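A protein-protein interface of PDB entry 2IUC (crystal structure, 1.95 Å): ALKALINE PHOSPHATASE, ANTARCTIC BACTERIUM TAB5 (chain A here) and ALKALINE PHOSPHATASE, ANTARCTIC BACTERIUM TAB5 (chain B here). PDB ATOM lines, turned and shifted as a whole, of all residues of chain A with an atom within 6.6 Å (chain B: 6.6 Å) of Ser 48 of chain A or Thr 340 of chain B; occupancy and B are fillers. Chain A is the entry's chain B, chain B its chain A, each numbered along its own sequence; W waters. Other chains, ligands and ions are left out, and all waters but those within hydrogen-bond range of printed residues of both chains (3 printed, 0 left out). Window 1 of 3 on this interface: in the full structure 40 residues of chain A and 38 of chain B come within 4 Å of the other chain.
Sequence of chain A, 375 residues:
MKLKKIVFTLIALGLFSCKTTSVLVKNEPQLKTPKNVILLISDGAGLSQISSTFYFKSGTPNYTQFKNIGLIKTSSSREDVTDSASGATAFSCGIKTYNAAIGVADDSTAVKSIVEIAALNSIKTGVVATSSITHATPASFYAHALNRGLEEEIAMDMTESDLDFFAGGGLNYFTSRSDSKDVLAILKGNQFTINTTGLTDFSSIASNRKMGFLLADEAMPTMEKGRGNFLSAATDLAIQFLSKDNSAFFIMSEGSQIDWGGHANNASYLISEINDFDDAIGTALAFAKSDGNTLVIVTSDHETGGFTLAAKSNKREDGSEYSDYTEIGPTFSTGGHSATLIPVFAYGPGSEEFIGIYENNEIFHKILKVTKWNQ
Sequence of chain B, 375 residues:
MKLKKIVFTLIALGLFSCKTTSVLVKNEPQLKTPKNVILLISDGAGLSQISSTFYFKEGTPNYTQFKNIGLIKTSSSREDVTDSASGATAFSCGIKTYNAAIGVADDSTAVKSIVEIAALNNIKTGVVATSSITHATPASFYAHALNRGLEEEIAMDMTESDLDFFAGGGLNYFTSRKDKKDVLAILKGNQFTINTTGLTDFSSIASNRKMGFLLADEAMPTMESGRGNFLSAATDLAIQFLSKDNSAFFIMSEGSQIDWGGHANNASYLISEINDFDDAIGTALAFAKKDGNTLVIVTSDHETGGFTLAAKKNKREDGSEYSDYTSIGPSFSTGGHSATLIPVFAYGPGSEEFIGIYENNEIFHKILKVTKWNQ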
ATOM      1  N   ALA A  45     -36.767  24.207 -21.541  1.00  0.00           N
ATOM      2  CA  ALA A  45     -35.863  23.261 -22.210  1.00  0.00           C
ATOM      3  C   ALA A  45     -35.929  23.294 -23.760  1.00  0.00           C
ATOM      4  O   ALA A  45     -36.847  22.673 -24.400  1.00  0.00           O
ATOM      5  CB  ALA A  45     -36.042  21.776 -21.705  1.00  0.00           C
ATOM      6  N   GLY A  46     -34.904  23.923 -24.357  1.00  0.00           N
ATOM      7  CA  GLY A  46     -34.675  23.727 -25.787  1.00  0.00           C
ATOM      8  C   GLY A  46     -33.978  22.432 -26.154  1.00  0.00           C
ATOM      9  O   GLY A  46     -33.665  21.553 -25.250  1.00  0.00           O
ATOM     10  N   LEU A  47     -33.699  22.253 -27.443  1.00  0.00           N
ATOM     11  CA  LEU A  47     -32.989  21.064 -27.839  1.00  0.00           C
ATOM     12  C   LEU A  47     -31.565  20.982 -27.181  1.00  0.00           C
ATOM     13  O   LEU A  47     -31.092  19.896 -26.923  1.00  0.00           O
ATOM     14  CB  LEU A  47     -32.882  20.955 -29.363  1.00  0.00           C
ATOM     15  CG  LEU A  47     -32.983  19.610 -30.101  1.00  0.00           C
ATOM     16  CD1 LEU A  47     -32.297  19.668 -31.422  1.00  0.00           C
ATOM     17  CD2 LEU A  47     -32.963  18.162 -29.305  1.00  0.00           C
ATOM     18  N   SER A  48     -30.888  22.099 -26.892  1.00  0.00           N
ATOM     19  CA  SER A  48     -29.552  21.983 -26.308  1.00  0.00           C
ATOM     20  C   SER A  48     -29.699  21.436 -24.873  1.00  0.00           C
ATOM     21  O   SER A  48     -28.946  20.597 -24.459  1.00  0.00           O
ATOM     22  CB  SER A  48     -28.914  23.376 -26.291  1.00  0.00           C
ATOM     23  OG  SER A  48     -28.408  23.746 -27.603  1.00  0.00           O
ATOM     24  N   GLN A  49     -30.681  21.921 -24.124  1.00  0.00           N
ATOM     25  CA  GLN A  49     -31.015  21.348 -22.770  1.00  0.00           C
ATOM     26  C   GLN A  49     -31.345  19.871 -22.797  1.00  0.00           C
ATOM     27  O   GLN A  49     -30.789  19.091 -22.006  1.00  0.00           O
ATOM     28  CB  GLN A  49     -32.204  22.108 -22.122  1.00  0.00           C
ATOM     29  CG  GLN A  49     -31.827  23.499 -21.634  1.00  0.00           C
ATOM     30  CD  GLN A  49     -31.986  24.559 -22.721  1.00  0.00           C
ATOM     31  OE1 GLN A  49     -32.194  24.260 -23.920  1.00  0.00           O
ATOM     32  NE2 GLN A  49     -31.919  25.794 -22.304  1.00  0.00           N
ATOM     33  N   ILE A  50     -32.242  19.458 -23.704  1.00  0.00           N
ATOM     34  CA  ILE A  50     -32.509  18.036 -23.898  1.00  0.00           C
ATOM     35  C   ILE A  50     -31.217  17.262 -24.196  1.00  0.00           C
ATOM     36  O   ILE A  50     -31.006  16.135 -23.731  1.00  0.00           O
ATOM     37  CB  ILE A  50     -33.509  17.864 -25.123  1.00  0.00           C
ATOM     38  CG1 ILE A  50     -34.881  18.487 -24.759  1.00  0.00           C
ATOM     39  CG2 ILE A  50     -33.603  16.417 -25.579  1.00  0.00           C
ATOM     40  CD1 ILE A  50     -35.860  18.557 -25.962  1.00  0.00           C
ATOM     41  N   SER A  51     -30.350  17.856 -25.026  1.00  0.00           N
ATOM     42  CA  SER A  51     -29.155  17.126 -25.488  1.00  0.00           C
ATOM     43  C   SER A  51     -28.179  16.888 -24.314  1.00  0.00           C
ATOM     44  O   SER A  51     -27.368  15.955 -24.339  1.00  0.00           O
ATOM     45  CB  SER A  51     -28.399  17.992 -26.520  1.00  0.00           C
ATOM     46  OG  SER A  51     -29.211  18.073 -27.672  1.00  0.00           O
ATOM     47  N   SER A  52     -28.258  17.731 -23.305  1.00  0.00           N
ATOM     48  CA  SER A  52     -27.337  17.567 -22.147  1.00  0.00           C
ATOM     49  C   SER A  52     -27.496  16.170 -21.485  1.00  0.00           C
ATOM     50  O   SER A  52     -26.536  15.665 -20.895  1.00  0.00           O
ATOM     51  CB  SER A  52     -27.500  18.730 -21.147  1.00  0.00           C
ATOM     52  OG  SER A  52     -28.728  18.606 -20.414  1.00  0.00           O
ATOM     53  N   THR A  53     -28.678  15.560 -21.564  1.00  0.00           N
ATOM     54  CA  THR A  53     -28.924  14.242 -20.955  1.00  0.00           C
ATOM     55  C   THR A  53     -28.162  13.167 -21.722  1.00  0.00           C
ATOM     56  O   THR A  53     -27.989  12.053 -21.232  1.00  0.00           O
ATOM     57  CB  THR A  53     -30.436  13.839 -20.968  1.00  0.00           C
ATOM     58  OG1 THR A  53     -30.950  13.751 -22.313  1.00  0.00           O
ATOM     59  CG2 THR A  53     -31.239  14.853 -20.221  1.00  0.00           C
ATOM     60  N   TYR A  55     -25.020  13.569 -22.547  1.00  0.00           N
ATOM     61  CA  TYR A  55     -23.628  13.692 -22.132  1.00  0.00           C
ATOM     62  C   TYR A  55     -23.407  13.747 -20.628  1.00  0.00           C
ATOM     63  O   TYR A  55     -22.249  13.568 -20.134  1.00  0.00           O
ATOM     64  CB  TYR A  55     -23.074  14.995 -22.756  1.00  0.00           C
ATOM     65  CG  TYR A  55     -23.044  14.911 -24.280  1.00  0.00           C
ATOM     66  CD1 TYR A  55     -24.108  15.427 -25.054  1.00  0.00           C
ATOM     67  CD2 TYR A  55     -21.962  14.319 -24.931  1.00  0.00           C
ATOM     68  CE1 TYR A  55     -24.094  15.377 -26.489  1.00  0.00           C
ATOM     69  CE2 TYR A  55     -21.921  14.239 -26.364  1.00  0.00           C
ATOM     70  CZ  TYR A  55     -23.011  14.771 -27.112  1.00  0.00           C
ATOM     71  OH  TYR A  55     -22.976  14.721 -28.453  1.00  0.00           O
ATOM     72  N   LEU A 270     -29.534  23.317 -13.962  1.00  0.00           N
ATOM     73  CA  LEU A 270     -30.317  23.009 -15.179  1.00  0.00           C
ATOM     74  C   LEU A 270     -30.253  21.515 -15.473  1.00  0.00           C
ATOM     75  O   LEU A 270     -31.311  20.806 -15.650  1.00  0.00           O
ATOM     76  CB  LEU A 270     -29.720  23.782 -16.378  1.00  0.00           C
ATOM     77  CG  LEU A 270     -30.482  23.724 -17.722  1.00  0.00           C
ATOM     78  CD1 LEU A 270     -30.051  25.082 -18.504  1.00  0.00           C
ATOM     79  CD2 LEU A 270     -30.142  22.433 -18.520  1.00  0.00           C
ATOM     80  N   ILE A 274     -33.176  18.614 -15.562  1.00  0.00           N
ATOM     81  CA  ILE A 274     -33.650  17.915 -16.756  1.00  0.00           C
ATOM     82  C   ILE A 274     -33.358  16.402 -16.722  1.00  0.00           C
ATOM     83  O   ILE A 274     -34.113  15.644 -17.296  1.00  0.00           O
ATOM     84  CB  ILE A 274     -33.229  18.606 -18.061  1.00  0.00           C
ATOM     85  CG1 ILE A 274     -34.080  18.059 -19.267  1.00  0.00           C
ATOM     86  CG2 ILE A 274     -31.709  18.526 -18.291  1.00  0.00           C
ATOM     87  CD1 ILE A 274     -33.806  18.905 -20.534  1.00  0.00           C
ATOM     88  N   GLU A 303     -37.430  27.910 -24.735  1.00  0.00           N
ATOM     89  CA  GLU A 303     -36.057  27.677 -24.330  1.00  0.00           C
ATOM     90  C   GLU A 303     -35.638  28.787 -23.392  1.00  0.00           C
ATOM     91  O   GLU A 303     -36.195  29.905 -23.452  1.00  0.00           O
ATOM     92  CB  GLU A 303     -35.105  27.618 -25.560  1.00  0.00           C
ATOM     93  CG  GLU A 303     -33.624  27.218 -25.235  1.00  0.00           C
ATOM     94  CD  GLU A 303     -32.624  28.327 -24.724  1.00  0.00           C
ATOM     95  OE1 GLU A 303     -32.905  29.574 -24.753  1.00  0.00           O
ATOM     96  OE2 GLU A 303     -31.528  27.875 -24.264  1.00  0.00           O
ATOM     97  N   GLY A 306     -30.135  30.549 -23.597  1.00  0.00           N
ATOM     98  CA  GLY A 306     -29.243  30.250 -24.708  1.00  0.00           C
ATOM     99  C   GLY A 306     -28.172  29.204 -24.299  1.00  0.00           C
ATOM    100  O   GLY A 306     -27.025  29.278 -24.722  1.00  0.00           O
ATOM    101  N   PHE A 307     -28.583  28.218 -23.484  1.00  0.00           N
ATOM    102  CA  PHE A 307     -27.736  27.094 -23.079  1.00  0.00           C
ATOM    103  C   PHE A 307     -27.104  26.357 -24.270  1.00  0.00           C
ATOM    104  O   PHE A 307     -27.804  25.994 -25.189  1.00  0.00           O
ATOM    105  CB  PHE A 307     -28.605  26.100 -22.299  1.00  0.00           C
ATOM    106  CG  PHE A 307     -27.878  24.905 -21.828  1.00  0.00           C
ATOM    107  CD1 PHE A 307     -26.955  25.014 -20.787  1.00  0.00           C
ATOM    108  CD2 PHE A 307     -28.152  23.644 -22.380  1.00  0.00           C
ATOM    109  CE1 PHE A 307     -26.295  23.891 -20.265  1.00  0.00           C
ATOM    110  CE2 PHE A 307     -27.491  22.504 -21.914  1.00  0.00           C
ATOM    111  CZ  PHE A 307     -26.559  22.611 -20.797  1.00  0.00           C
ATOM    112  N   THR A 308     -25.768  26.143 -24.242  1.00  0.00           N
ATOM    113  CA  THR A 308     -25.012  25.622 -25.367  1.00  0.00           C
ATOM    114  C   THR A 308     -23.975  24.636 -24.870  1.00  0.00           C
ATOM    115  O   THR A 308     -23.249  24.924 -23.826  1.00  0.00           O
ATOM    116  CB  THR A 308     -24.313  26.838 -26.067  1.00  0.00           C
ATOM    117  OG1 THR A 308     -25.317  27.751 -26.462  1.00  0.00           O
ATOM    118  CG2 THR A 308     -23.529  26.439 -27.295  1.00  0.00           C
ATOM    119  N   LEU A 309     -23.870  23.485 -25.551  1.00  0.00           N
ATOM    120  CA  LEU A 309     -22.904  22.443 -25.119  1.00  0.00           C
ATOM    121  C   LEU A 309     -21.571  22.762 -25.829  1.00  0.00           C
ATOM    122  O   LEU A 309     -21.149  22.016 -26.696  1.00  0.00           O
ATOM    123  CB  LEU A 309     -23.418  21.035 -25.445  1.00  0.00           C
ATOM    124  CG  LEU A 309     -24.795  20.760 -24.775  1.00  0.00           C
ATOM    125  CD1 LEU A 309     -25.286  19.389 -25.239  1.00  0.00           C
ATOM    126  CD2 LEU A 309     -24.527  20.717 -23.280  1.00  0.00           C
ATOM    127  N   GLY B  46     -27.821  24.513 -35.858  1.00  0.00           N
ATOM    128  CA  GLY B  46     -28.691  23.817 -34.933  1.00  0.00           C
ATOM    129  C   GLY B  46     -30.128  24.343 -35.187  1.00  0.00           C
ATOM    130  O   GLY B  46     -30.414  25.217 -36.079  1.00  0.00           O
ATOM    131  N   LEU B  47     -31.022  23.796 -34.385  1.00  0.00           N
ATOM    132  CA  LEU B  47     -32.471  24.226 -34.338  1.00  0.00           C
ATOM    133  C   LEU B  47     -32.690  25.707 -34.151  1.00  0.00           C
ATOM    134  O   LEU B  47     -33.645  26.282 -34.686  1.00  0.00           O
ATOM    135  CB  LEU B  47     -33.190  23.449 -33.225  1.00  0.00           C
ATOM    136  CG  LEU B  47     -34.738  23.587 -33.279  1.00  0.00           C
ATOM    137  CD1 LEU B  47     -35.293  23.403 -34.740  1.00  0.00           C
ATOM    138  CD2 LEU B  47     -35.251  22.477 -32.232  1.00  0.00           C
ATOM    139  N   SER B  48     -31.817  26.379 -33.366  1.00  0.00           N
ATOM    140  CA  SER B  48     -31.938  27.818 -33.198  1.00  0.00           C
ATOM    141  C   SER B  48     -31.673  28.572 -34.496  1.00  0.00           C
ATOM    142  O   SER B  48     -32.385  29.520 -34.805  1.00  0.00           O
ATOM    143  CB  SER B  48     -30.951  28.388 -32.095  1.00  0.00           C
ATOM    144  OG  SER B  48     -31.311  27.908 -30.774  1.00  0.00           O
ATOM    145  N   ILE B  72     -30.080  13.706 -34.626  1.00  0.00           N
ATOM    146  CA  ILE B  72     -28.794  12.979 -34.580  1.00  0.00           C
ATOM    147  C   ILE B  72     -27.831  13.453 -33.498  1.00  0.00           C
ATOM    148  O   ILE B  72     -27.708  14.633 -33.252  1.00  0.00           O
ATOM    149  CB  ILE B  72     -28.040  13.045 -35.969  1.00  0.00           C
ATOM    150  CG1 ILE B  72     -27.894  14.508 -36.499  1.00  0.00           C
ATOM    151  CG2 ILE B  72     -28.674  12.088 -36.976  1.00  0.00           C
ATOM    152  CD1 ILE B  72     -26.970  14.584 -37.848  1.00  0.00           C
ATOM    153  N   LYS B  73     -27.095  12.511 -32.898  1.00  0.00           N
ATOM    154  CA  LYS B  73     -25.948  12.802 -32.017  1.00  0.00           C
ATOM    155  C   LYS B  73     -24.656  12.886 -32.866  1.00  0.00           C
ATOM    156  O   LYS B  73     -24.329  11.922 -33.609  1.00  0.00           O
ATOM    157  CB  LYS B  73     -25.849  11.705 -30.900  1.00  0.00           C
ATOM    158  CG  LYS B  73     -24.851  12.084 -29.830  1.00  0.00           C
ATOM    159  CD  LYS B  73     -24.788  10.964 -28.767  1.00  0.00           C
ATOM    160  CE  LYS B  73     -23.703  11.337 -27.597  1.00  0.00           C
ATOM    161  NZ  LYS B  73     -23.668  10.145 -26.587  1.00  0.00           N
ATOM    162  N   THR B  74     -23.943  13.992 -32.733  1.00  0.00           N
ATOM    163  CA  THR B  74     -22.921  14.398 -33.703  1.00  0.00           C
ATOM    164  C   THR B  74     -21.449  14.199 -33.205  1.00  0.00           C
ATOM    165  O   THR B  74     -20.525  14.435 -33.966  1.00  0.00           O
ATOM    166  CB  THR B  74     -23.023  15.870 -34.064  1.00  0.00           C
ATOM    167  OG1 THR B  74     -22.823  16.669 -32.883  1.00  0.00           O
ATOM    168  CG2 THR B  74     -24.445  16.170 -34.723  1.00  0.00           C
ATOM    169  N   ASP B 301     -24.150  19.211 -39.902  1.00  0.00           N
ATOM    170  CA  ASP B 301     -23.109  18.450 -39.216  1.00  0.00           C
ATOM    171  C   ASP B 301     -22.981  18.660 -37.703  1.00  0.00           C
ATOM    172  O   ASP B 301     -22.540  17.739 -36.988  1.00  0.00           O
ATOM    173  CB  ASP B 301     -21.744  18.627 -39.915  1.00  0.00           C
ATOM    174  CG  ASP B 301     -21.333  20.126 -40.114  1.00  0.00           C
ATOM    175  OD1 ASP B 301     -22.068  21.095 -39.788  1.00  0.00           O
ATOM    176  OD2 ASP B 301     -20.149  20.345 -40.473  1.00  0.00           O
ATOM    177  N   HIS B 302     -23.316  19.851 -37.189  1.00  0.00           N
ATOM    178  CA  HIS B 302     -23.193  20.228 -35.772  1.00  0.00           C
ATOM    179  C   HIS B 302     -23.714  21.687 -35.767  1.00  0.00           C
ATOM    180  O   HIS B 302     -23.998  22.274 -36.840  1.00  0.00           O
ATOM    181  CB  HIS B 302     -21.685  20.185 -35.299  1.00  0.00           C
ATOM    182  CG  HIS B 302     -20.828  21.054 -36.184  1.00  0.00           C
ATOM    183  ND1 HIS B 302     -20.862  22.431 -36.108  1.00  0.00           N
ATOM    184  CD2 HIS B 302     -20.055  20.768 -37.248  1.00  0.00           C
ATOM    185  CE1 HIS B 302     -20.168  22.953 -37.087  1.00  0.00           C
ATOM    186  NE2 HIS B 302     -19.644  21.968 -37.779  1.00  0.00           N
ATOM    187  N   GLU B 303     -23.852  22.257 -34.567  1.00  0.00           N
ATOM    188  CA  GLU B 303     -24.238  23.623 -34.332  1.00  0.00           C
ATOM    189  C   GLU B 303     -22.991  24.493 -34.136  1.00  0.00           C
ATOM    190  O   GLU B 303     -21.966  24.003 -33.640  1.00  0.00           O
ATOM    191  CB  GLU B 303     -25.011  23.664 -33.009  1.00  0.00           C
ATOM    192  CG  GLU B 303     -25.751  24.964 -32.838  1.00  0.00           C
ATOM    193  CD  GLU B 303     -24.983  26.115 -32.079  1.00  0.00           C
ATOM    194  OE1 GLU B 303     -23.920  25.884 -31.410  1.00  0.00           O
ATOM    195  OE2 GLU B 303     -25.540  27.240 -32.082  1.00  0.00           O
ATOM    196  N   THR B 304     -23.082  25.760 -34.497  1.00  0.00           N
ATOM    197  CA  THR B 304     -21.969  26.690 -34.190  1.00  0.00           C
ATOM    198  C   THR B 304     -22.357  28.049 -33.549  1.00  0.00           C
ATOM    199  O   THR B 304     -23.295  28.767 -34.009  1.00  0.00           O
ATOM    200  CB  THR B 304     -21.234  27.091 -35.470  1.00  0.00           C
ATOM    201  OG1 THR B 304     -20.861  25.927 -36.166  1.00  0.00           O
ATOM    202  CG2 THR B 304     -19.877  27.950 -35.123  1.00  0.00           C
ATOM    203  N   SER B 338     -20.792  23.377 -31.163  1.00  0.00           N
ATOM    204  CA  SER B 338     -21.368  22.781 -29.954  1.00  0.00           C
ATOM    205  C   SER B 338     -21.942  21.371 -30.196  1.00  0.00           C
ATOM    206  O   SER B 338     -22.082  20.965 -31.347  1.00  0.00           O
ATOM    207  CB  SER B 338     -22.392  23.720 -29.312  1.00  0.00           C
ATOM    208  OG  SER B 338     -23.590  23.830 -30.073  1.00  0.00           O
ATOM    209  N   ALA B 339     -22.297  20.673 -29.107  1.00  0.00           N
ATOM    210  CA  ALA B 339     -22.577  19.252 -29.171  1.00  0.00           C
ATOM    211  C   ALA B 339     -24.052  18.941 -29.149  1.00  0.00           C
ATOM    212  O   ALA B 339     -24.490  17.806 -28.857  1.00  0.00           O
ATOM    213  CB  ALA B 339     -21.855  18.501 -28.071  1.00  0.00           C
ATOM    214  N   THR B 340     -24.830  19.958 -29.411  1.00  0.00           N
ATOM    215  CA  THR B 340     -26.299  19.730 -29.387  1.00  0.00           C
ATOM    216  C   THR B 340     -26.644  18.593 -30.364  1.00  0.00           C
ATOM    217  O   THR B 340     -25.988  18.448 -31.440  1.00  0.00           O
ATOM    218  CB  THR B 340     -27.114  21.037 -29.594  1.00  0.00           C
ATOM    219  OG1 THR B 340     -28.534  20.769 -29.502  1.00  0.00           O
ATOM    220  CG2 THR B 340     -26.763  21.731 -30.917  1.00  0.00           C
ATOM    221  N   LEU B 341     -27.700  17.824 -30.054  1.00  0.00           N
ATOM    222  CA  LEU B 341     -28.320  17.001 -31.086  1.00  0.00           C
ATOM    223  C   LEU B 341     -28.797  17.916 -32.211  1.00  0.00           C
ATOM    224  O   LEU B 341     -29.192  19.023 -31.941  1.00  0.00           O
ATOM    225  CB  LEU B 341     -29.546  16.279 -30.582  1.00  0.00           C
ATOM    226  CG  LEU B 341     -29.410  15.222 -29.497  1.00  0.00           C
ATOM    227  CD1 LEU B 341     -30.781  14.572 -29.232  1.00  0.00           C
ATOM    228  CD2 LEU B 341     -28.429  14.221 -29.796  1.00  0.00           C
ATOM    229  N   ILE B 342     -28.883  17.398 -33.441  1.00  0.00           N
ATOM    230  CA  ILE B 342     -29.176  18.228 -34.619  1.00  0.00           C
ATOM    231  C   ILE B 342     -30.449  17.628 -35.320  1.00  0.00           C
ATOM    232  O   ILE B 342     -30.587  16.423 -35.433  1.00  0.00           O
ATOM    233  CB  ILE B 342     -27.979  18.155 -35.579  1.00  0.00           C
ATOM    234  CG1 ILE B 342     -26.724  18.941 -35.005  1.00  0.00           C
ATOM    235  CG2 ILE B 342     -28.399  18.492 -37.003  1.00  0.00           C
ATOM    236  CD1 ILE B 342     -26.885  20.424 -34.798  1.00  0.00           C
HETATM  237  O   HOH W   1     -24.874  15.628 -30.483  1.00  0.00           O
HETATM  238  O   HOH W   2     -25.531  23.299 -27.867  1.00  0.00           O
HETATM  239  O   HOH W   3     -30.056  23.402 -30.316  1.00  0.00           O
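Ser 48 of chain A touches just one residue of chain B: Thr 340 (3.5 Å). Of the printed residues of chain B, Tyr 55 of chain A touches Lys 73 (3.5 Å) and Ala 339 (3.4 Å). Gly 306 of chain A touches none of the printed residues of chain B. Gly 46 of chain B touches none of the printed residues of chain A. Of the printed residues of chain A, Ser 338 of chain B touches Thr 308 (3.6 Å) and Leu 309 (3.4 Å). Of the printed residues of chain A, Thr 340 of chain B touches Leu 47, Ser 48 and Ser 51. The nearest printed residue of chain A that does not touch Leu 341 of chain B is Ile 50 of chain A (5.0 Å).
Water W1 lies within hydrogen-bond range of O of Ala 339 of chain B, OH of Tyr 55 of chain A, N of Thr 74 of chain B and O of Thr 340 of chain B. Water W2 lies within hydrogen-bond range of N of Leu 309 of chain A (2.9 Å), OG of Ser 48 of chain A (2.9 Å) and OG of Ser 338 of chain B (3.0 Å). Water W3 bridges OG1 of Thr 340 of chain B and OG of Ser 48 of chain A.
The side-chain carboxylate (OE1) of Glu 303 of chain B lies within hydrogen-bond range of the side-chain hydroxyl (OG) of Ser 338 of chain B (2.5 Å). OG of Ser 51 of chain A lies within hydrogen-bond range of O of Leu 47 of chain A (2.7 Å). O of Phe 307 of chain A lies close to OG of Ser 48 of chain A. OG1 of Thr 308 of chain A lies within hydrogen-bond range of O of Gly 306 of chain A (2.9 Å).
Of the 15 printed residues of chain B, 5 touch a printed residue of chain A. Printed residues of chain B that touch a printed residue of chain A: Lys 73, Ser 338, Ala 339, Thr 340 and Leu 341. Of the 17 printed residues of chain A, 6 touch a printed residue of chain B. Hydrophobic or aromatic side chains of chain A that line the printed part of chain B: Leu 47, Tyr 55 and Leu 309. Among the printed residues, 10 pairs touch across the chains.
The side-chain hydroxyl (OH) of Tyr 55 of chain A lies close to the backbone carbonyl oxygen (O) of Ala 339 of chain B (3.5 Å). The backbone NH (N) of Ala 339 of chain B lies within hydrogen-bond range of the backbone carbonyl oxygen (O) of Leu 309 of chain A (3.0 Å). The side-chain hydroxyl (OG1) of Thr 340 of chain B is in hydrogen-bond range of the side-chain hydroxyl (OG) of Ser 51 of chain A (3.3 Å). N of Leu 341 of chain B lies within hydrogen-bond range of OG of Ser 51 of chain A (2.8 Å).
Among the printed residues, pairs that only touch across the chains: Leu 47 of chain A with Leu 341 of chain B, Leu 309 of chain A with Ser 338 of chain B, Tyr 55 of chain A with Lys 73 of chain B, Ser 48 of chain A with Thr 340 of chain B, Thr 308 of chain A with Ser 338 of chain B and Leu 47 of chain A with Thr 340 of chain B.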
